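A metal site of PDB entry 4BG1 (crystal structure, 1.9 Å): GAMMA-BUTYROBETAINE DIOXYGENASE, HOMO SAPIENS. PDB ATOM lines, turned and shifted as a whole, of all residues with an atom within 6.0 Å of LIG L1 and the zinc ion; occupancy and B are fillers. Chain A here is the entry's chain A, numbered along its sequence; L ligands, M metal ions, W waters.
O4 of LIG L1 is in salt-bridge range of NH2 of Arg 360 (2.8 Å).
NH1 of Arg 349 is in salt-bridge range of O5 of LIG L1.
The side-chain amide nitrogen (ND2) of Asn 191 sits at hydrogen-bond distance from an oxygen (O2) of LG2 L2, 3.0 Å away.
NE2 of Gln 215 is in hydrogen-bond range of OD2 of Asp 204 (3.2 Å).
The side-chain carboxylate (OD2) of Asp 204 lies within hydrogen-bond range of the side-chain hydroxyl (OH) of Tyr 366, at 2.5 Å.
The guanidinium group (NH2) of Arg 360 sits at hydrogen-bond distance from the backbone carbonyl oxygen (O) of Gly 227, 2.9 Å away.
NH1 of Arg 349 sits at hydrogen-bond distance from O of Ala 193 (3.0 Å).
O of Arg 349 lies within hydrogen-bond range of N of Leu 199 (2.9 Å).
N of Ala 193 lies within hydrogen-bond range of OD1 of Asn 191.
The backbone carbonyl oxygen (O) of Leu 362 sits at hydrogen-bond distance from the backbone NH (N) of Val 183, 2.8 Å away.
Residues that only touch LIG L1: Val 183, Ala 193, Leu 199 and Leu 362.
Within 4 Å of LIG L1: Val 183, Ala 193, Leu 199, His 202, Asp 204, His 347, Arg 349, Arg 360 and Leu 362.
The nearest printed residue that does not touch LIG L1 is Leu 217 (4.01 Å).
Of the 22 residues printed, 3 come within 4 Å of the zinc ion.
The zinc ion is bound by O2 of LIG L1 (2.0 Å), OD1 of Asp 204 (2.1 Å), NE2 of His 202 (2.1 Å), NE2 of His 347 (2.2 Å) and O3 of LIG L1 (2.2 Å).
Water W1 lies within hydrogen-bond range of an oxygen (O4) of LIG L1 (2.7 Å), the side-chain hydroxyl (OG) of Ser 229 (2.8 Å) and the backbone carbonyl oxygen (O) of Gly 348 (3.1 Å).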
ATOM      1  N   TRP A 181      19.340  12.693 -35.767  1.00  0.00           N
ATOM      2  CA  TRP A 181      20.676  13.145 -36.153  1.00  0.00           C
ATOM      3  C   TRP A 181      21.745  12.446 -35.330  1.00  0.00           C
ATOM      4  O   TRP A 181      21.493  12.010 -34.186  1.00  0.00           O
ATOM      5  CB  TRP A 181      20.814  14.680 -36.064  1.00  0.00           C
ATOM      6  CG  TRP A 181      19.894  15.319 -35.102  1.00  0.00           C
ATOM      7  CD1 TRP A 181      18.665  15.837 -35.374  1.00  0.00           C
ATOM      8  CD2 TRP A 181      20.117  15.527 -33.697  1.00  0.00           C
ATOM      9  NE1 TRP A 181      18.103  16.352 -34.223  1.00  0.00           N
ATOM     10  CE2 TRP A 181      18.955  16.154 -33.181  1.00  0.00           C
ATOM     11  CE3 TRP A 181      21.166  15.224 -32.830  1.00  0.00           C
ATOM     12  CZ2 TRP A 181      18.831  16.502 -31.838  1.00  0.00           C
ATOM     13  CZ3 TRP A 181      21.037  15.574 -31.500  1.00  0.00           C
ATOM     14  CH2 TRP A 181      19.872  16.215 -31.019  1.00  0.00           C
ATOM     15  N   VAL A 183      25.202  12.504 -33.370  1.00  0.00           N
ATOM     16  CA  VAL A 183      26.233  13.301 -32.720  1.00  0.00           C
ATOM     17  C   VAL A 183      27.525  12.500 -32.679  1.00  0.00           C
ATOM     18  O   VAL A 183      27.649  11.564 -31.900  1.00  0.00           O
ATOM     19  CB  VAL A 183      25.817  13.769 -31.302  1.00  0.00           C
ATOM     20  CG1 VAL A 183      26.822  14.750 -30.737  1.00  0.00           C
ATOM     21  CG2 VAL A 183      24.427  14.368 -31.316  1.00  0.00           C
ATOM     22  N   ASN A 191      28.362  21.810 -37.696  1.00  0.00           N
ATOM     23  CA  ASN A 191      27.893  22.243 -36.370  1.00  0.00           C
ATOM     24  C   ASN A 191      28.976  21.900 -35.355  1.00  0.00           C
ATOM     25  O   ASN A 191      29.591  20.829 -35.442  1.00  0.00           O
ATOM     26  CB  ASN A 191      26.573  21.520 -36.038  1.00  0.00           C
ATOM     27  CG  ASN A 191      25.821  22.153 -34.863  1.00  0.00           C
ATOM     28  OD1 ASN A 191      26.199  21.995 -33.703  1.00  0.00           O
ATOM     29  ND2 ASN A 191      24.744  22.845 -35.170  1.00  0.00           N
ATOM     30  N   ALA A 193      28.703  20.767 -32.500  1.00  0.00           N
ATOM     31  CA  ALA A 193      28.365  19.523 -31.802  1.00  0.00           C
ATOM     32  C   ALA A 193      29.005  18.308 -32.456  1.00  0.00           C
ATOM     33  O   ALA A 193      29.290  17.298 -31.791  1.00  0.00           O
ATOM     34  CB  ALA A 193      26.846  19.363 -31.740  1.00  0.00           C
ATOM     35  N   TYR A 194      29.254  18.424 -33.752  1.00  0.00           N
ATOM     36  CA  TYR A 194      29.808  17.326 -34.533  1.00  0.00           C
ATOM     37  C   TYR A 194      31.353  17.379 -34.575  1.00  0.00           C
ATOM     38  O   TYR A 194      31.976  17.064 -35.581  1.00  0.00           O
ATOM     39  CB  TYR A 194      29.218  17.328 -35.952  1.00  0.00           C
ATOM     40  CG  TYR A 194      27.712  17.140 -36.050  1.00  0.00           C
ATOM     41  CD1 TYR A 194      26.993  16.436 -35.078  1.00  0.00           C
ATOM     42  CD2 TYR A 194      27.013  17.597 -37.168  1.00  0.00           C
ATOM     43  CE1 TYR A 194      25.629  16.259 -35.186  1.00  0.00           C
ATOM     44  CE2 TYR A 194      25.640  17.421 -37.280  1.00  0.00           C
ATOM     45  CZ  TYR A 194      24.953  16.742 -36.293  1.00  0.00           C
ATOM     46  OH  TYR A 194      23.618  16.549 -36.398  1.00  0.00           O
ATOM     47  N   LEU A 199      31.199  21.407 -25.282  1.00  0.00           N
ATOM     48  CA  LEU A 199      30.040  22.267 -25.513  1.00  0.00           C
ATOM     49  C   LEU A 199      29.688  22.843 -24.162  1.00  0.00           C
ATOM     50  O   LEU A 199      29.382  22.088 -23.206  1.00  0.00           O
ATOM     51  CB  LEU A 199      28.844  21.498 -26.086  1.00  0.00           C
ATOM     52  CG  LEU A 199      29.096  20.731 -27.400  1.00  0.00           C
ATOM     53  CD1 LEU A 199      27.877  19.918 -27.797  1.00  0.00           C
ATOM     54  CD2 LEU A 199      29.446  21.716 -28.496  1.00  0.00           C
ATOM     55  N   HIS A 202      24.186  25.351 -23.314  1.00  0.00           N
ATOM     56  CA  HIS A 202      23.341  25.934 -24.354  1.00  0.00           C
ATOM     57  C   HIS A 202      21.969  25.261 -24.366  1.00  0.00           C
ATOM     58  O   HIS A 202      21.802  24.159 -23.828  1.00  0.00           O
ATOM     59  CB  HIS A 202      23.981  25.743 -25.726  1.00  0.00           C
ATOM     60  CG  HIS A 202      24.111  24.308 -26.129  1.00  0.00           C
ATOM     61  ND1 HIS A 202      25.043  23.473 -25.573  1.00  0.00           N
ATOM     62  CD2 HIS A 202      23.410  23.554 -27.009  1.00  0.00           C
ATOM     63  CE1 HIS A 202      24.936  22.261 -26.116  1.00  0.00           C
ATOM     64  NE2 HIS A 202      23.952  22.301 -26.991  1.00  0.00           N
ATOM     65  N   THR A 203      21.004  25.926 -24.996  1.00  0.00           N
ATOM     66  CA  THR A 203      19.753  25.339 -25.470  1.00  0.00           C
ATOM     67  C   THR A 203      19.959  25.019 -26.929  1.00  0.00           C
ATOM     68  O   THR A 203      20.724  25.695 -27.580  1.00  0.00           O
ATOM     69  CB  THR A 203      18.556  26.290 -25.318  1.00  0.00           C
ATOM     70  OG1 THR A 203      18.787  27.521 -26.033  1.00  0.00           O
ATOM     71  CG2 THR A 203      18.327  26.630 -23.825  1.00  0.00           C
ATOM     72  N   ASP A 204      19.280  24.003 -27.439  1.00  0.00           N
ATOM     73  CA  ASP A 204      19.383  23.686 -28.869  1.00  0.00           C
ATOM     74  C   ASP A 204      18.461  24.528 -29.730  1.00  0.00           C
ATOM     75  O   ASP A 204      17.291  24.748 -29.416  1.00  0.00           O
ATOM     76  CB  ASP A 204      19.083  22.224 -29.155  1.00  0.00           C
ATOM     77  CG  ASP A 204      20.300  21.327 -29.041  1.00  0.00           C
ATOM     78  OD1 ASP A 204      21.272  21.692 -28.352  1.00  0.00           O
ATOM     79  OD2 ASP A 204      20.268  20.245 -29.690  1.00  0.00           O
ATOM     80  N   GLN A 215      14.050  17.539 -26.067  1.00  0.00           N
ATOM     81  CA  GLN A 215      15.144  16.920 -26.769  1.00  0.00           C
ATOM     82  C   GLN A 215      15.364  15.475 -26.243  1.00  0.00           C
ATOM     83  O   GLN A 215      15.247  15.208 -25.054  1.00  0.00           O
ATOM     84  CB  GLN A 215      16.426  17.742 -26.574  1.00  0.00           C
ATOM     85  CG  GLN A 215      17.653  17.194 -27.267  1.00  0.00           C
ATOM     86  CD  GLN A 215      18.802  18.207 -27.375  1.00  0.00           C
ATOM     87  OE1 GLN A 215      19.948  17.840 -27.604  1.00  0.00           O
ATOM     88  NE2 GLN A 215      18.499  19.464 -27.181  1.00  0.00           N
ATOM     89  N   LEU A 217      18.256  12.375 -26.393  1.00  0.00           N
ATOM     90  CA  LEU A 217      19.630  11.953 -26.725  1.00  0.00           C
ATOM     91  C   LEU A 217      19.902  10.553 -26.219  1.00  0.00           C
ATOM     92  O   LEU A 217      19.826  10.288 -25.021  1.00  0.00           O
ATOM     93  CB  LEU A 217      20.694  12.859 -26.101  1.00  0.00           C
ATOM     94  CG  LEU A 217      20.981  14.247 -26.631  1.00  0.00           C
ATOM     95  CD1 LEU A 217      22.069  14.904 -25.780  1.00  0.00           C
ATOM     96  CD2 LEU A 217      21.440  14.162 -28.076  1.00  0.00           C
ATOM     97  N   GLY A 227      33.749  13.483 -22.548  1.00  0.00           N
ATOM     98  CA  GLY A 227      32.391  13.375 -23.072  1.00  0.00           C
ATOM     99  C   GLY A 227      31.300  13.219 -22.032  1.00  0.00           C
ATOM    100  O   GLY A 227      30.184  12.843 -22.370  1.00  0.00           O
ATOM    101  N   ASP A 228      31.613  13.539 -20.770  1.00  0.00           N
ATOM    102  CA  ASP A 228      30.586  13.656 -19.704  1.00  0.00           C
ATOM    103  C   ASP A 228      29.550  14.722 -20.060  1.00  0.00           C
ATOM    104  O   ASP A 228      29.866  15.705 -20.752  1.00  0.00           O
ATOM    105  CB  ASP A 228      31.208  14.062 -18.349  1.00  0.00           C
ATOM    106  CG  ASP A 228      32.384  13.194 -17.944  1.00  0.00           C
ATOM    107  OD1 ASP A 228      33.417  13.223 -18.627  1.00  0.00           O
ATOM    108  OD2 ASP A 228      32.240  12.451 -16.945  1.00  0.00           O
ATOM    109  N   SER A 229      28.332  14.555 -19.545  1.00  0.00           N
ATOM    110  CA  SER A 229      27.220  15.474 -19.730  1.00  0.00           C
ATOM    111  C   SER A 229      27.075  16.378 -18.539  1.00  0.00           C
ATOM    112  O   SER A 229      27.429  16.005 -17.417  1.00  0.00           O
ATOM    113  CB  SER A 229      25.939  14.662 -19.924  1.00  0.00           C
ATOM    114  OG  SER A 229      26.064  13.824 -21.045  1.00  0.00           O
ATOM    115  N   MET A 332      26.772   9.493 -19.690  1.00  0.00           N
ATOM    116  CA  MET A 332      25.915   8.530 -20.372  1.00  0.00           C
ATOM    117  C   MET A 332      26.687   7.270 -20.754  1.00  0.00           C
ATOM    118  O   MET A 332      27.849   7.345 -21.165  1.00  0.00           O
ATOM    119  CB  MET A 332      25.321   9.168 -21.635  1.00  0.00           C
ATOM    120  CG  MET A 332      24.487  10.396 -21.350  1.00  0.00           C
ATOM    121  SD  MET A 332      23.462  10.909 -22.753  1.00  0.00           S
ATOM    122  CE  MET A 332      22.185   9.673 -22.655  1.00  0.00           C
ATOM    123  N   PHE A 340      14.665  15.665 -22.187  1.00  0.00           N
ATOM    124  CA  PHE A 340      14.655  16.847 -21.358  1.00  0.00           C
ATOM    125  C   PHE A 340      13.962  18.031 -22.013  1.00  0.00           C
ATOM    126  O   PHE A 340      13.746  18.049 -23.244  1.00  0.00           O
ATOM    127  CB  PHE A 340      16.085  17.170 -20.850  1.00  0.00           C
ATOM    128  CG  PHE A 340      17.097  17.414 -21.948  1.00  0.00           C
ATOM    129  CD1 PHE A 340      17.291  18.692 -22.447  1.00  0.00           C
ATOM    130  CD2 PHE A 340      17.854  16.380 -22.442  1.00  0.00           C
ATOM    131  CE1 PHE A 340      18.218  18.919 -23.441  1.00  0.00           C
ATOM    132  CE2 PHE A 340      18.785  16.607 -23.446  1.00  0.00           C
ATOM    133  CZ  PHE A 340      18.961  17.878 -23.954  1.00  0.00           C
ATOM    134  N   HIS A 347      22.244  22.492 -21.431  1.00  0.00           N
ATOM    135  CA  HIS A 347      23.034  21.291 -21.395  1.00  0.00           C
ATOM    136  C   HIS A 347      24.358  21.508 -22.068  1.00  0.00           C
ATOM    137  O   HIS A 347      24.547  22.478 -22.853  1.00  0.00           O
ATOM    138  CB  HIS A 347      22.268  20.146 -22.015  1.00  0.00           C
ATOM    139  CG  HIS A 347      21.977  20.309 -23.478  1.00  0.00           C
ATOM    140  ND1 HIS A 347      20.974  21.137 -23.956  1.00  0.00           N
ATOM    141  CD2 HIS A 347      22.553  19.756 -24.579  1.00  0.00           C
ATOM    142  CE1 HIS A 347      20.936  21.065 -25.271  1.00  0.00           C
ATOM    143  NE2 HIS A 347      21.898  20.255 -25.675  1.00  0.00           N
ATOM    144  N   GLY A 348      25.298  20.624 -21.765  1.00  0.00           N
ATOM    145  CA  GLY A 348      26.649  20.723 -22.307  1.00  0.00           C
ATOM    146  C   GLY A 348      27.364  19.388 -22.241  1.00  0.00           C
ATOM    147  O   GLY A 348      26.815  18.384 -21.805  1.00  0.00           O
ATOM    148  N   ARG A 349      28.583  19.381 -22.738  1.00  0.00           N
ATOM    149  CA  ARG A 349      29.387  18.203 -22.649  1.00  0.00           C
ATOM    150  C   ARG A 349      30.871  18.547 -22.558  1.00  0.00           C
ATOM    151  O   ARG A 349      31.341  19.564 -23.109  1.00  0.00           O
ATOM    152  CB  ARG A 349      29.164  17.263 -23.838  1.00  0.00           C
ATOM    153  CG  ARG A 349      29.693  17.763 -25.137  1.00  0.00           C
ATOM    154  CD  ARG A 349      30.197  16.667 -26.074  1.00  0.00           C
ATOM    155  NE  ARG A 349      30.875  17.338 -27.165  1.00  0.00           N
ATOM    156  CZ  ARG A 349      30.493  17.375 -28.441  1.00  0.00           C
ATOM    157  NH1 ARG A 349      29.413  16.718 -28.879  1.00  0.00           N
ATOM    158  NH2 ARG A 349      31.233  18.074 -29.292  1.00  0.00           N
ATOM    159  N   ARG A 360      32.590   7.696 -30.045  1.00  0.00           N
ATOM    160  CA  ARG A 360      31.483   8.285 -29.328  1.00  0.00           C
ATOM    161  C   ARG A 360      30.396   8.628 -30.333  1.00  0.00           C
ATOM    162  O   ARG A 360      30.671   9.222 -31.363  1.00  0.00           O
ATOM    163  CB  ARG A 360      31.926   9.550 -28.591  1.00  0.00           C
ATOM    164  CG  ARG A 360      30.870  10.069 -27.652  1.00  0.00           C
ATOM    165  CD  ARG A 360      31.335  11.313 -26.950  1.00  0.00           C
ATOM    166  NE  ARG A 360      30.435  11.755 -25.873  1.00  0.00           N
ATOM    167  CZ  ARG A 360      29.433  12.641 -25.995  1.00  0.00           C
ATOM    168  NH1 ARG A 360      29.110  13.197 -27.154  1.00  0.00           N
ATOM    169  NH2 ARG A 360      28.723  12.973 -24.918  1.00  0.00           N
ATOM    170  N   LEU A 362      26.060   9.566 -30.241  1.00  0.00           N
ATOM    171  CA  LEU A 362      24.714   9.711 -29.702  1.00  0.00           C
ATOM    172  C   LEU A 362      23.755   9.857 -30.873  1.00  0.00           C
ATOM    173  O   LEU A 362      24.128  10.463 -31.866  1.00  0.00           O
ATOM    174  CB  LEU A 362      24.599  10.933 -28.799  1.00  0.00           C
ATOM    175  CG  LEU A 362      25.683  11.259 -27.769  1.00  0.00           C
ATOM    176  CD1 LEU A 362      25.281  12.530 -27.024  1.00  0.00           C
ATOM    177  CD2 LEU A 362      25.883  10.129 -26.781  1.00  0.00           C
ATOM    178  N   TYR A 366      14.040  15.667 -31.592  1.00  0.00           N
ATOM    179  CA  TYR A 366      13.262  16.675 -30.897  1.00  0.00           C
ATOM    180  C   TYR A 366      11.765  16.331 -30.961  1.00  0.00           C
ATOM    181  O   TYR A 366      11.333  15.619 -31.868  1.00  0.00           O
ATOM    182  CB  TYR A 366      13.444  18.052 -31.566  1.00  0.00           C
ATOM    183  CG  TYR A 366      14.864  18.572 -31.623  1.00  0.00           C
ATOM    184  CD1 TYR A 366      15.569  18.841 -30.453  1.00  0.00           C
ATOM    185  CD2 TYR A 366      15.482  18.867 -32.840  1.00  0.00           C
ATOM    186  CE1 TYR A 366      16.866  19.326 -30.480  1.00  0.00           C
ATOM    187  CE2 TYR A 366      16.788  19.353 -32.885  1.00  0.00           C
ATOM    188  CZ  TYR A 366      17.468  19.603 -31.694  1.00  0.00           C
ATOM    189  OH  TYR A 366      18.771  20.084 -31.686  1.00  0.00           O
HETATM  190  C1  LIG L   1      24.201  18.668 -29.146  1.00  0.00           C
HETATM  191  C2  LIG L   1      24.636  18.341 -27.796  1.00  0.00           C
HETATM  192  C3  LIG L   1      25.595  16.757 -26.249  1.00  0.00           C
HETATM  193  C4  LIG L   1      26.662  15.672 -26.277  1.00  0.00           C
HETATM  194  O1  LIG L   1      24.477  17.860 -30.074  1.00  0.00           O
HETATM  195  O2  LIG L   1      23.545  19.728 -29.311  1.00  0.00           O
HETATM  196  O3  LIG L   1      24.295  19.078 -26.879  1.00  0.00           O
HETATM  197  O4  LIG L   1      26.932  15.112 -25.199  1.00  0.00           O
HETATM  198  N1  LIG L   1      25.328  17.242 -27.604  1.00  0.00           N
HETATM  199  O5  LIG L   1      27.220  15.384 -27.347  1.00  0.00           O
HETATM  200  C1  LG2 L   2      22.198  18.399 -32.834  1.00  0.00           C
HETATM  201  C2  LG2 L   2      23.661  18.161 -33.110  1.00  0.00           C
HETATM  202  C3  LG2 L   2      24.139  19.299 -33.986  1.00  0.00           C
HETATM  203  C4  LG2 L   2      22.873  19.771 -34.675  1.00  0.00           C
HETATM  204  C5  LG2 L   2      20.465  19.380 -34.275  1.00  0.00           C
HETATM  205  C6  LG2 L   2      21.779  20.563 -32.586  1.00  0.00           C
HETATM  206  C7  LG2 L   2      21.537  21.974 -32.934  1.00  0.00           C
HETATM  207  C8  LG2 L   2      22.274  22.773 -31.826  1.00  0.00           C
HETATM  208  C9  LG2 L   2      22.207  24.155 -32.369  1.00  0.00           C
HETATM  209  N1  LG2 L   2      21.797  19.575 -33.662  1.00  0.00           N
HETATM  210  O1  LG2 L   2      21.673  25.065 -31.782  1.00  0.00           O
HETATM  211  O2  LG2 L   2      22.719  24.312 -33.561  1.00  0.00           O
HETATM  212 ZN    ZN M   1      22.878  20.571 -27.583  1.00  0.00          ZN
HETATM  213  O   HOH W   1      25.619  15.836 -23.004  1.00  0.00           O
